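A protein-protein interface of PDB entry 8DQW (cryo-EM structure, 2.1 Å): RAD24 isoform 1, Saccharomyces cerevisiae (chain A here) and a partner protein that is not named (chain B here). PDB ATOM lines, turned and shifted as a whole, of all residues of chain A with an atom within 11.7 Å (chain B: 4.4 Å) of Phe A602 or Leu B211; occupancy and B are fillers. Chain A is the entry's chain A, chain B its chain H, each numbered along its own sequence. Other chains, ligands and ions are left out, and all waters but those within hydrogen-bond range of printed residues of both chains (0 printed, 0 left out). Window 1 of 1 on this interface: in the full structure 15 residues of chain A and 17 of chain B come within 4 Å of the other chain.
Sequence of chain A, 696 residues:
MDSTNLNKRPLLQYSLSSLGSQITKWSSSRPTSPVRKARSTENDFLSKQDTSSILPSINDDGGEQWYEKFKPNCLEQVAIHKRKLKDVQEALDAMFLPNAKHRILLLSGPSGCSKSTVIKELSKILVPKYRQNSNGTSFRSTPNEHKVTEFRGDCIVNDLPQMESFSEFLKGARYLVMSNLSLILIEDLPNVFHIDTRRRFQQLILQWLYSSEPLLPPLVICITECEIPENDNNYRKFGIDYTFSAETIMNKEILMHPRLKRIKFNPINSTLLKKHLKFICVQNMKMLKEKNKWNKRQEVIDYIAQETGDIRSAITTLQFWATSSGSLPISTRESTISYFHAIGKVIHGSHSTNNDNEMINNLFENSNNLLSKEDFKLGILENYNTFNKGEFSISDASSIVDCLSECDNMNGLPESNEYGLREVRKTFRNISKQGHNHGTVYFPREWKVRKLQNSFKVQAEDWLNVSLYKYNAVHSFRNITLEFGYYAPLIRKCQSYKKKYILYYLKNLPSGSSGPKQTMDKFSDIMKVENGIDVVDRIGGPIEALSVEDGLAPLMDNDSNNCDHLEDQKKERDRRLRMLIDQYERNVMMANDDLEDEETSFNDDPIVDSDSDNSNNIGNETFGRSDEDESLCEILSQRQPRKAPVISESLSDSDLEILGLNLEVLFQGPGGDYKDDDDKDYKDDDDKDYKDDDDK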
ATOM      1  N   VAL A 588     -22.531  33.808  37.106  1.00  0.00           N
ATOM      2  CA  VAL A 588     -22.584  32.356  36.947  1.00  0.00           C
ATOM      3  C   VAL A 588     -22.076  31.955  35.568  1.00  0.00           C
ATOM      4  O   VAL A 588     -21.276  31.023  35.427  1.00  0.00           O
ATOM      5  CB  VAL A 588     -24.015  31.841  37.192  1.00  0.00           C
ATOM      6  CG1 VAL A 588     -24.054  30.322  37.116  1.00  0.00           C
ATOM      7  CG2 VAL A 588     -24.533  32.326  38.540  1.00  0.00           C
ATOM      8  N   MET A 589     -22.534  32.654  34.526  1.00  0.00           N
ATOM      9  CA  MET A 589     -22.125  32.303  33.170  1.00  0.00           C
ATOM     10  C   MET A 589     -20.692  32.736  32.883  1.00  0.00           C
ATOM     11  O   MET A 589     -20.022  32.128  32.040  1.00  0.00           O
ATOM     12  CB  MET A 589     -23.078  32.933  32.153  1.00  0.00           C
ATOM     13  CG  MET A 589     -24.186  32.004  31.675  1.00  0.00           C
ATOM     14  SD  MET A 589     -24.590  32.238  29.933  1.00  0.00           S
ATOM     15  CE  MET A 589     -23.462  31.075  29.167  1.00  0.00           C
ATOM     16  N   MET A 590     -20.207  33.776  33.565  1.00  0.00           N
ATOM     17  CA  MET A 590     -18.850  34.252  33.319  1.00  0.00           C
ATOM     18  C   MET A 590     -17.828  33.168  33.637  1.00  0.00           C
ATOM     19  O   MET A 590     -16.914  32.909  32.846  1.00  0.00           O
ATOM     20  CB  MET A 590     -18.591  35.515  34.148  1.00  0.00           C
ATOM     21  CG  MET A 590     -17.140  35.730  34.586  1.00  0.00           C
ATOM     22  SD  MET A 590     -15.980  36.038  33.234  1.00  0.00           S
ATOM     23  CE  MET A 590     -16.938  37.090  32.146  1.00  0.00           C
ATOM     24  N   ALA A 591     -17.971  32.520  34.790  1.00  0.00           N
ATOM     25  CA  ALA A 591     -17.061  31.459  35.200  1.00  0.00           C
ATOM     26  C   ALA A 591     -17.578  30.862  36.502  1.00  0.00           C
ATOM     27  O   ALA A 591     -18.320  31.507  37.248  1.00  0.00           O
ATOM     28  CB  ALA A 591     -15.628  31.970  35.383  1.00  0.00           C
ATOM     29  N   ASN A 592     -17.173  29.621  36.762  1.00  0.00           N
ATOM     30  CA  ASN A 592     -17.510  28.923  37.992  1.00  0.00           C
ATOM     31  C   ASN A 592     -16.254  28.284  38.563  1.00  0.00           C
ATOM     32  O   ASN A 592     -15.353  27.880  37.822  1.00  0.00           O
ATOM     33  CB  ASN A 592     -18.584  27.852  37.758  1.00  0.00           C
ATOM     34  CG  ASN A 592     -19.983  28.433  37.684  1.00  0.00           C
ATOM     35  OD1 ASN A 592     -20.298  29.413  38.362  1.00  0.00           O
ATOM     36  ND2 ASN A 592     -20.832  27.831  36.860  1.00  0.00           N
ATOM     37  N   ASP A 593     -16.200  28.197  39.894  1.00  0.00           N
ATOM     38  CA  ASP A 593     -15.024  27.626  40.542  1.00  0.00           C
ATOM     39  C   ASP A 593     -14.834  26.166  40.148  1.00  0.00           C
ATOM     40  O   ASP A 593     -13.710  25.734  39.868  1.00  0.00           O
ATOM     41  CB  ASP A 593     -15.140  27.774  42.061  1.00  0.00           C
ATOM     42  CG  ASP A 593     -16.000  26.697  42.694  1.00  0.00           C
ATOM     43  OD1 ASP A 593     -15.478  25.591  42.951  1.00  0.00           O
ATOM     44  OD2 ASP A 593     -17.197  26.956  42.934  1.00  0.00           O
ATOM     45  N   ASP A 594     -15.923  25.396  40.105  1.00  0.00           N
ATOM     46  CA  ASP A 594     -15.868  23.988  39.727  1.00  0.00           C
ATOM     47  C   ASP A 594     -14.746  23.275  40.478  1.00  0.00           C
ATOM     48  O   ASP A 594     -14.743  23.252  41.713  1.00  0.00           O
ATOM     49  CB  ASP A 594     -15.690  23.858  38.212  1.00  0.00           C
ATOM     50  CG  ASP A 594     -16.856  24.440  37.438  1.00  0.00           C
ATOM     51  OD1 ASP A 594     -17.936  24.625  38.036  1.00  0.00           O
ATOM     52  OD2 ASP A 594     -16.692  24.714  36.230  1.00  0.00           O
ATOM     53  N   LEU A 595     -13.794  22.691  39.752  1.00  0.00           N
ATOM     54  CA  LEU A 595     -12.653  22.004  40.341  1.00  0.00           C
ATOM     55  C   LEU A 595     -11.392  22.407  39.586  1.00  0.00           C
ATOM     56  O   LEU A 595     -11.438  23.156  38.607  1.00  0.00           O
ATOM     57  CB  LEU A 595     -12.846  20.482  40.313  1.00  0.00           C
ATOM     58  CG  LEU A 595     -14.123  19.960  40.974  1.00  0.00           C
ATOM     59  CD1 LEU A 595     -14.369  18.509  40.591  1.00  0.00           C
ATOM     60  CD2 LEU A 595     -14.047  20.112  42.485  1.00  0.00           C
ATOM     61  N   GLU A 596     -10.252  21.901  40.051  1.00  0.00           N
ATOM     62  CA  GLU A 596      -8.966  22.193  39.434  1.00  0.00           C
ATOM     63  C   GLU A 596      -8.710  21.213  38.297  1.00  0.00           C
ATOM     64  O   GLU A 596      -8.760  19.994  38.495  1.00  0.00           O
ATOM     65  CB  GLU A 596      -7.842  22.112  40.468  1.00  0.00           C
ATOM     66  CG  GLU A 596      -8.065  22.988  41.692  1.00  0.00           C
ATOM     67  CD  GLU A 596      -6.937  22.878  42.701  1.00  0.00           C
ATOM     68  OE1 GLU A 596      -7.002  21.984  43.571  1.00  0.00           O
ATOM     69  OE2 GLU A 596      -5.987  23.685  42.623  1.00  0.00           O
ATOM     70  N   ASP A 597      -8.436  21.750  37.108  1.00  0.00           N
ATOM     71  CA  ASP A 597      -8.196  20.924  35.930  1.00  0.00           C
ATOM     72  C   ASP A 597      -6.954  21.397  35.186  1.00  0.00           C
ATOM     73  O   ASP A 597      -6.249  22.299  35.650  1.00  0.00           O
ATOM     74  CB  ASP A 597      -9.412  20.949  35.003  1.00  0.00           C
ATOM     75  CG  ASP A 597     -10.716  20.726  35.744  1.00  0.00           C
ATOM     76  OD1 ASP A 597     -10.967  19.582  36.176  1.00  0.00           O
ATOM     77  OD2 ASP A 597     -11.488  21.696  35.896  1.00  0.00           O
ATOM     78  N   GLU A 598      -6.680  20.792  34.029  1.00  0.00           N
ATOM     79  CA  GLU A 598      -5.506  21.136  33.228  1.00  0.00           C
ATOM     80  C   GLU A 598      -5.877  22.281  32.288  1.00  0.00           C
ATOM     81  O   GLU A 598      -6.132  22.100  31.095  1.00  0.00           O
ATOM     82  CB  GLU A 598      -5.003  19.917  32.464  1.00  0.00           C
ATOM     83  CG  GLU A 598      -4.522  18.785  33.357  1.00  0.00           C
ATOM     84  CD  GLU A 598      -4.056  17.577  32.568  1.00  0.00           C
ATOM     85  OE1 GLU A 598      -4.102  17.626  31.320  1.00  0.00           O
ATOM     86  OE2 GLU A 598      -3.645  16.578  33.195  1.00  0.00           O
ATOM     87  N   GLU A 599      -5.904  23.490  32.852  1.00  0.00           N
ATOM     88  CA  GLU A 599      -6.216  24.670  32.052  1.00  0.00           C
ATOM     89  C   GLU A 599      -5.135  24.945  31.015  1.00  0.00           C
ATOM     90  O   GLU A 599      -5.438  25.420  29.915  1.00  0.00           O
ATOM     91  CB  GLU A 599      -6.403  25.885  32.961  1.00  0.00           C
ATOM     92  CG  GLU A 599      -7.625  25.794  33.862  1.00  0.00           C
ATOM     93  CD  GLU A 599      -7.748  26.979  34.799  1.00  0.00           C
ATOM     94  OE1 GLU A 599      -6.780  27.762  34.902  1.00  0.00           O
ATOM     95  OE2 GLU A 599      -8.813  27.128  35.434  1.00  0.00           O
ATOM     96  N   THR A 600      -3.872  24.663  31.347  1.00  0.00           N
ATOM     97  CA  THR A 600      -2.800  24.842  30.374  1.00  0.00           C
ATOM     98  C   THR A 600      -3.014  23.952  29.156  1.00  0.00           C
ATOM     99  O   THR A 600      -2.815  24.388  28.016  1.00  0.00           O
ATOM    100  CB  THR A 600      -1.448  24.545  31.022  1.00  0.00           C
ATOM    101  OG1 THR A 600      -1.445  23.210  31.542  1.00  0.00           O
ATOM    102  CG2 THR A 600      -1.166  25.528  32.148  1.00  0.00           C
ATOM    103  N   SER A 601      -3.422  22.701  29.378  1.00  0.00           N
ATOM    104  CA  SER A 601      -3.720  21.814  28.258  1.00  0.00           C
ATOM    105  C   SER A 601      -4.881  22.350  27.431  1.00  0.00           C
ATOM    106  O   SER A 601      -4.870  22.262  26.198  1.00  0.00           O
ATOM    107  CB  SER A 601      -4.033  20.408  28.772  1.00  0.00           C
ATOM    108  OG  SER A 601      -4.191  19.497  27.699  1.00  0.00           O
ATOM    109  N   PHE A 602      -5.897  22.908  28.093  1.00  0.00           N
ATOM    110  CA  PHE A 602      -7.011  23.508  27.366  1.00  0.00           C
ATOM    111  C   PHE A 602      -6.535  24.662  26.494  1.00  0.00           C
ATOM    112  O   PHE A 602      -6.993  24.822  25.356  1.00  0.00           O
ATOM    113  CB  PHE A 602      -8.080  23.984  28.348  1.00  0.00           C
ATOM    114  CG  PHE A 602      -9.410  24.261  27.709  1.00  0.00           C
ATOM    115  CD1 PHE A 602      -9.658  25.479  27.096  1.00  0.00           C
ATOM    116  CD2 PHE A 602     -10.413  23.308  27.721  1.00  0.00           C
ATOM    117  CE1 PHE A 602     -10.879  25.738  26.508  1.00  0.00           C
ATOM    118  CE2 PHE A 602     -11.637  23.562  27.134  1.00  0.00           C
ATOM    119  CZ  PHE A 602     -11.871  24.779  26.526  1.00  0.00           C
ATOM    120  N   ASN A 603      -5.621  25.483  27.012  1.00  0.00           N
ATOM    121  CA  ASN A 603      -5.071  26.577  26.221  1.00  0.00           C
ATOM    122  C   ASN A 603      -4.113  26.085  25.143  1.00  0.00           C
ATOM    123  O   ASN A 603      -3.803  26.840  24.216  1.00  0.00           O
ATOM    124  CB  ASN A 603      -4.356  27.577  27.131  1.00  0.00           C
ATOM    125  CG  ASN A 603      -4.079  28.899  26.440  1.00  0.00           C
ATOM    126  OD1 ASN A 603      -4.836  29.328  25.570  1.00  0.00           O
ATOM    127  ND2 ASN A 603      -2.989  29.552  26.827  1.00  0.00           N
ATOM    128  N   ASP A 604      -3.636  24.841  25.243  1.00  0.00           N
ATOM    129  CA  ASP A 604      -2.701  24.308  24.259  1.00  0.00           C
ATOM    130  C   ASP A 604      -3.368  23.953  22.937  1.00  0.00           C
ATOM    131  O   ASP A 604      -2.659  23.677  21.964  1.00  0.00           O
ATOM    132  CB  ASP A 604      -1.997  23.072  24.824  1.00  0.00           C
ATOM    133  CG  ASP A 604      -0.995  23.416  25.911  1.00  0.00           C
ATOM    134  OD1 ASP A 604      -0.599  24.596  26.007  1.00  0.00           O
ATOM    135  OD2 ASP A 604      -0.605  22.504  26.670  1.00  0.00           O
ATOM    136  N   ASP A 605      -4.698  23.951  22.876  1.00  0.00           N
ATOM    137  CA  ASP A 605      -5.443  23.661  21.650  1.00  0.00           C
ATOM    138  C   ASP A 605      -6.444  24.787  21.412  1.00  0.00           C
ATOM    139  O   ASP A 605      -7.658  24.606  21.562  1.00  0.00           O
ATOM    140  CB  ASP A 605      -6.135  22.300  21.737  1.00  0.00           C
ATOM    141  CG  ASP A 605      -7.143  22.224  22.868  1.00  0.00           C
ATOM    142  OD1 ASP A 605      -6.819  22.674  23.984  1.00  0.00           O
ATOM    143  OD2 ASP A 605      -8.260  21.712  22.637  1.00  0.00           O
ATOM    144  N   PRO A 606      -5.961  25.968  21.030  1.00  0.00           N
ATOM    145  CA  PRO A 606      -6.863  27.109  20.854  1.00  0.00           C
ATOM    146  C   PRO A 606      -7.823  26.907  19.693  1.00  0.00           C
ATOM    147  O   PRO A 606      -7.547  26.170  18.742  1.00  0.00           O
ATOM    148  CB  PRO A 606      -5.908  28.278  20.590  1.00  0.00           C
ATOM    149  CG  PRO A 606      -4.683  27.640  20.030  1.00  0.00           C
ATOM    150  CD  PRO A 606      -4.564  26.315  20.723  1.00  0.00           C
ATOM    151  N   ILE A 607      -8.971  27.583  19.785  1.00  0.00           N
ATOM    152  CA  ILE A 607      -9.971  27.497  18.732  1.00  0.00           C
ATOM    153  C   ILE A 607      -9.404  28.050  17.427  1.00  0.00           C
ATOM    154  O   ILE A 607      -8.586  28.979  17.418  1.00  0.00           O
ATOM    155  CB  ILE A 607     -11.247  28.253  19.139  1.00  0.00           C
ATOM    156  CG1 ILE A 607     -12.434  27.800  18.286  1.00  0.00           C
ATOM    157  CG2 ILE A 607     -11.038  29.755  19.010  1.00  0.00           C
ATOM    158  CD1 ILE A 607     -13.672  28.647  18.466  1.00  0.00           C
ATOM    159  N   VAL A 608      -9.845  27.468  16.314  1.00  0.00           N
ATOM    160  CA  VAL A 608      -9.461  27.909  14.979  1.00  0.00           C
ATOM    161  C   VAL A 608     -10.731  28.215  14.197  1.00  0.00           C
ATOM    162  O   VAL A 608     -11.665  27.405  14.179  1.00  0.00           O
ATOM    163  CB  VAL A 608      -8.608  26.854  14.246  1.00  0.00           C
ATOM    164  CG1 VAL A 608      -7.497  26.348  15.155  1.00  0.00           C
ATOM    165  CG2 VAL A 608      -9.471  25.696  13.765  1.00  0.00           C
ATOM    166  N   THR B  92     -17.063  18.905  24.325  1.00  0.00           N
ATOM    167  CA  THR B  92     -18.185  19.082  25.235  1.00  0.00           C
ATOM    168  C   THR B  92     -18.390  20.562  25.526  1.00  0.00           C
ATOM    169  O   THR B  92     -17.422  21.308  25.706  1.00  0.00           O
ATOM    170  CB  THR B  92     -17.953  18.324  26.544  1.00  0.00           C
ATOM    171  OG1 THR B  92     -17.400  17.033  26.261  1.00  0.00           O
ATOM    172  CG2 THR B  92     -19.261  18.158  27.307  1.00  0.00           C
ATOM    173  N   MET B  93     -19.653  20.983  25.567  1.00  0.00           N
ATOM    174  CA  MET B  93     -19.987  22.372  25.838  1.00  0.00           C
ATOM    175  C   MET B  93     -21.313  22.446  26.579  1.00  0.00           C
ATOM    176  O   MET B  93     -22.101  21.499  26.584  1.00  0.00           O
ATOM    177  CB  MET B  93     -20.070  23.195  24.547  1.00  0.00           C
ATOM    178  CG  MET B  93     -20.821  22.500  23.427  1.00  0.00           C
ATOM    179  SD  MET B  93     -21.503  23.649  22.216  1.00  0.00           S
ATOM    180  CE  MET B  93     -20.028  24.129  21.324  1.00  0.00           C
ATOM    181  N   LEU B 123     -18.055  27.514  15.785  1.00  0.00           N
ATOM    182  CA  LEU B 123     -17.600  27.979  17.089  1.00  0.00           C
ATOM    183  C   LEU B 123     -16.606  29.114  16.889  1.00  0.00           C
ATOM    184  O   LEU B 123     -15.675  28.994  16.085  1.00  0.00           O
ATOM    185  CB  LEU B 123     -16.958  26.839  17.881  1.00  0.00           C
ATOM    186  CG  LEU B 123     -16.748  27.100  19.374  1.00  0.00           C
ATOM    187  CD1 LEU B 123     -18.080  27.128  20.110  1.00  0.00           C
ATOM    188  CD2 LEU B 123     -15.822  26.056  19.977  1.00  0.00           C
ATOM    189  N   ASN B 151     -12.386  27.604  32.121  1.00  0.00           N
ATOM    190  CA  ASN B 151     -13.504  27.388  31.211  1.00  0.00           C
ATOM    191  C   ASN B 151     -13.821  28.659  30.429  1.00  0.00           C
ATOM    192  O   ASN B 151     -14.775  29.367  30.752  1.00  0.00           O
ATOM    193  CB  ASN B 151     -14.740  26.923  31.984  1.00  0.00           C
ATOM    194  CG  ASN B 151     -14.896  27.631  33.315  1.00  0.00           C
ATOM    195  OD1 ASN B 151     -14.383  28.733  33.510  1.00  0.00           O
ATOM    196  ND2 ASN B 151     -15.609  26.998  34.240  1.00  0.00           N
ATOM    197  N   PRO B 152     -13.020  28.953  29.406  1.00  0.00           N
ATOM    198  CA  PRO B 152     -13.288  30.139  28.583  1.00  0.00           C
ATOM    199  C   PRO B 152     -14.645  30.051  27.901  1.00  0.00           C
ATOM    200  O   PRO B 152     -15.114  28.973  27.532  1.00  0.00           O
ATOM    201  CB  PRO B 152     -12.145  30.131  27.560  1.00  0.00           C
ATOM    202  CG  PRO B 152     -11.077  29.287  28.171  1.00  0.00           C
ATOM    203  CD  PRO B 152     -11.785  28.263  29.000  1.00  0.00           C
ATOM    204  N   CYS B 154     -17.060  30.965  24.771  1.00  0.00           N
ATOM    205  CA  CYS B 154     -17.023  31.210  23.336  1.00  0.00           C
ATOM    206  C   CYS B 154     -18.441  31.498  22.842  1.00  0.00           C
ATOM    207  O   CYS B 154     -19.390  31.578  23.627  1.00  0.00           O
ATOM    208  CB  CYS B 154     -16.399  30.016  22.610  1.00  0.00           C
ATOM    209  SG  CYS B 154     -15.144  29.140  23.572  1.00  0.00           S
ATOM    210  N   VAL B 209     -21.548  30.204  24.990  1.00  0.00           N
ATOM    211  CA  VAL B 209     -21.341  28.787  25.260  1.00  0.00           C
ATOM    212  C   VAL B 209     -20.100  28.653  26.129  1.00  0.00           C
ATOM    213  O   VAL B 209     -19.176  29.466  26.047  1.00  0.00           O
ATOM    214  CB  VAL B 209     -21.203  27.978  23.946  1.00  0.00           C
ATOM    215  CG1 VAL B 209     -20.512  26.647  24.195  1.00  0.00           C
ATOM    216  CG2 VAL B 209     -22.567  27.764  23.310  1.00  0.00           C
ATOM    217  N   LYS B 210     -20.083  27.623  26.974  1.00  0.00           N
ATOM    218  CA  LYS B 210     -18.967  27.371  27.879  1.00  0.00           C
ATOM    219  C   LYS B 210     -18.413  25.979  27.614  1.00  0.00           C
ATOM    220  O   LYS B 210     -19.116  24.984  27.806  1.00  0.00           O
ATOM    221  CB  LYS B 210     -19.406  27.504  29.339  1.00  0.00           C
ATOM    222  CG  LYS B 210     -18.274  27.350  30.343  1.00  0.00           C
ATOM    223  CD  LYS B 210     -18.759  27.554  31.769  1.00  0.00           C
ATOM    224  CE  LYS B 210     -19.376  26.284  32.333  1.00  0.00           C
ATOM    225  NZ  LYS B 210     -19.791  26.448  33.754  1.00  0.00           N
ATOM    226  N   LEU B 211     -17.158  25.909  27.182  1.00  0.00           N
ATOM    227  CA  LEU B 211     -16.534  24.621  26.924  1.00  0.00           C
ATOM    228  C   LEU B 211     -16.220  23.905  28.234  1.00  0.00           C
ATOM    229  O   LEU B 211     -16.052  24.523  29.290  1.00  0.00           O
ATOM    230  CB  LEU B 211     -15.258  24.797  26.101  1.00  0.00           C
ATOM    231  CG  LEU B 211     -15.441  24.720  24.584  1.00  0.00           C
ATOM    232  CD1 LEU B 211     -16.450  25.755  24.109  1.00  0.00           C
ATOM    233  CD2 LEU B 211     -14.108  24.902  23.875  1.00  0.00           C
ATOM    234  N   LEU B 212     -16.140  22.578  28.155  1.00  0.00           N
ATOM    235  CA  LEU B 212     -15.922  21.729  29.315  1.00  0.00           C
ATOM    236  C   LEU B 212     -14.651  20.909  29.136  1.00  0.00           C
ATOM    237  O   LEU B 212     -14.229  20.623  28.012  1.00  0.00           O
ATOM    238  CB  LEU B 212     -17.113  20.790  29.548  1.00  0.00           C
ATOM    239  CG  LEU B 212     -18.166  21.276  30.547  1.00  0.00           C
ATOM    240  CD1 LEU B 212     -18.914  22.482  30.000  1.00  0.00           C
ATOM    241  CD2 LEU B 212     -19.133  20.154  30.890  1.00  0.00           C
ATOM    242  N   PHE B 213     -14.047  20.536  30.259  1.00  0.00           N
ATOM    243  CA  PHE B 213     -12.839  19.728  30.261  1.00  0.00           C
ATOM    244  C   PHE B 213     -13.192  18.242  30.235  1.00  0.00           C
ATOM    245  O   PHE B 213     -14.353  17.846  30.352  1.00  0.00           O
ATOM    246  CB  PHE B 213     -11.984  20.047  31.489  1.00  0.00           C
ATOM    247  CG  PHE B 213     -11.529  21.477  31.559  1.00  0.00           C
ATOM    248  CD1 PHE B 213     -12.401  22.478  31.955  1.00  0.00           C
ATOM    249  CD2 PHE B 213     -10.229  21.820  31.232  1.00  0.00           C
ATOM    250  CE1 PHE B 213     -11.985  23.793  32.021  1.00  0.00           C
ATOM    251  CE2 PHE B 213      -9.806  23.134  31.297  1.00  0.00           C
ATOM    252  CZ  PHE B 213     -10.686  24.122  31.692  1.00  0.00           C
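The side-chain amide oxygen (OD1) of Asn A592 lies close to the backbone carbonyl oxygen (O) of Val A588, 3.5 Å away.
The backbone carbonyl oxygen of Phe A602 lies close to the side-chain carboxylate of Asp A605 (2.6 Å).
Hydrophobic or aromatic side chains of chain A that line the printed part of chain B: Ala A591, Phe A602 and Ile A607.
Of the 11 printed residues of chain B, 6 touch a printed residue of chain A.
Hydrophobic or aromatic side chains of chain B within 4 Å of the printed part of chain A: Leu B123, Pro B152, Leu B211 and Phe B213.
Of the printed residues of chain B, Asn A592 touches Asn B151 (3.7 Å) and Lys B210 (3.6 Å).
Asp A593 touches none of the printed residues of chain B.
Of the printed residues of chain B, Asp A594 touches Asn B151.
Of the printed residues of chain B, Asp A597 touches Phe B213.
Thr A600 touches none of the printed residues of chain B.
Of the printed residues of chain B, Phe A602 touches Pro B152 (3.7 Å), Leu B211 (3.4 Å) and Phe B213 (3.5 Å).
Printed residues of chain B within 4 Å of Ile A607: Leu B123.
No residue of chain A comes within 4 Å of Thr B92.
No residue of chain A comes within 4 Å of Met B93.
Printed residues of chain A within 4 Å of Leu B123: Ile A607 (3.1 Å).
No residue of chain A comes within 4 Å of Cys B154.
Leu B211 touches one residue of chain A.
The nearest printed residue of chain B that does not touch Phe A602 is Leu B212 (4.02 Å).
Among the printed residues, pairs that only touch across the chains: Ala A591 with Asn B151 (3.9 Å), Asn A592 with Asn B151 (3.7 Å), Asn A592 with Lys B210 (3.6 Å), Asp A597 with Phe B213 (3.96 Å), Glu A598 with Phe B213 (3.8 Å), Glu A599 with Phe B213 (3.98 Å), Phe A602 with Pro B152 (3.7 Å), Phe A602 with Leu B211 (3.4 Å), Phe A602 with Phe B213 (3.5 Å) and Ile A607 with Leu B123 (3.1 Å).
ND2 of Asn B151 lies within hydrogen-bond range of OD2 of Asp A594.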
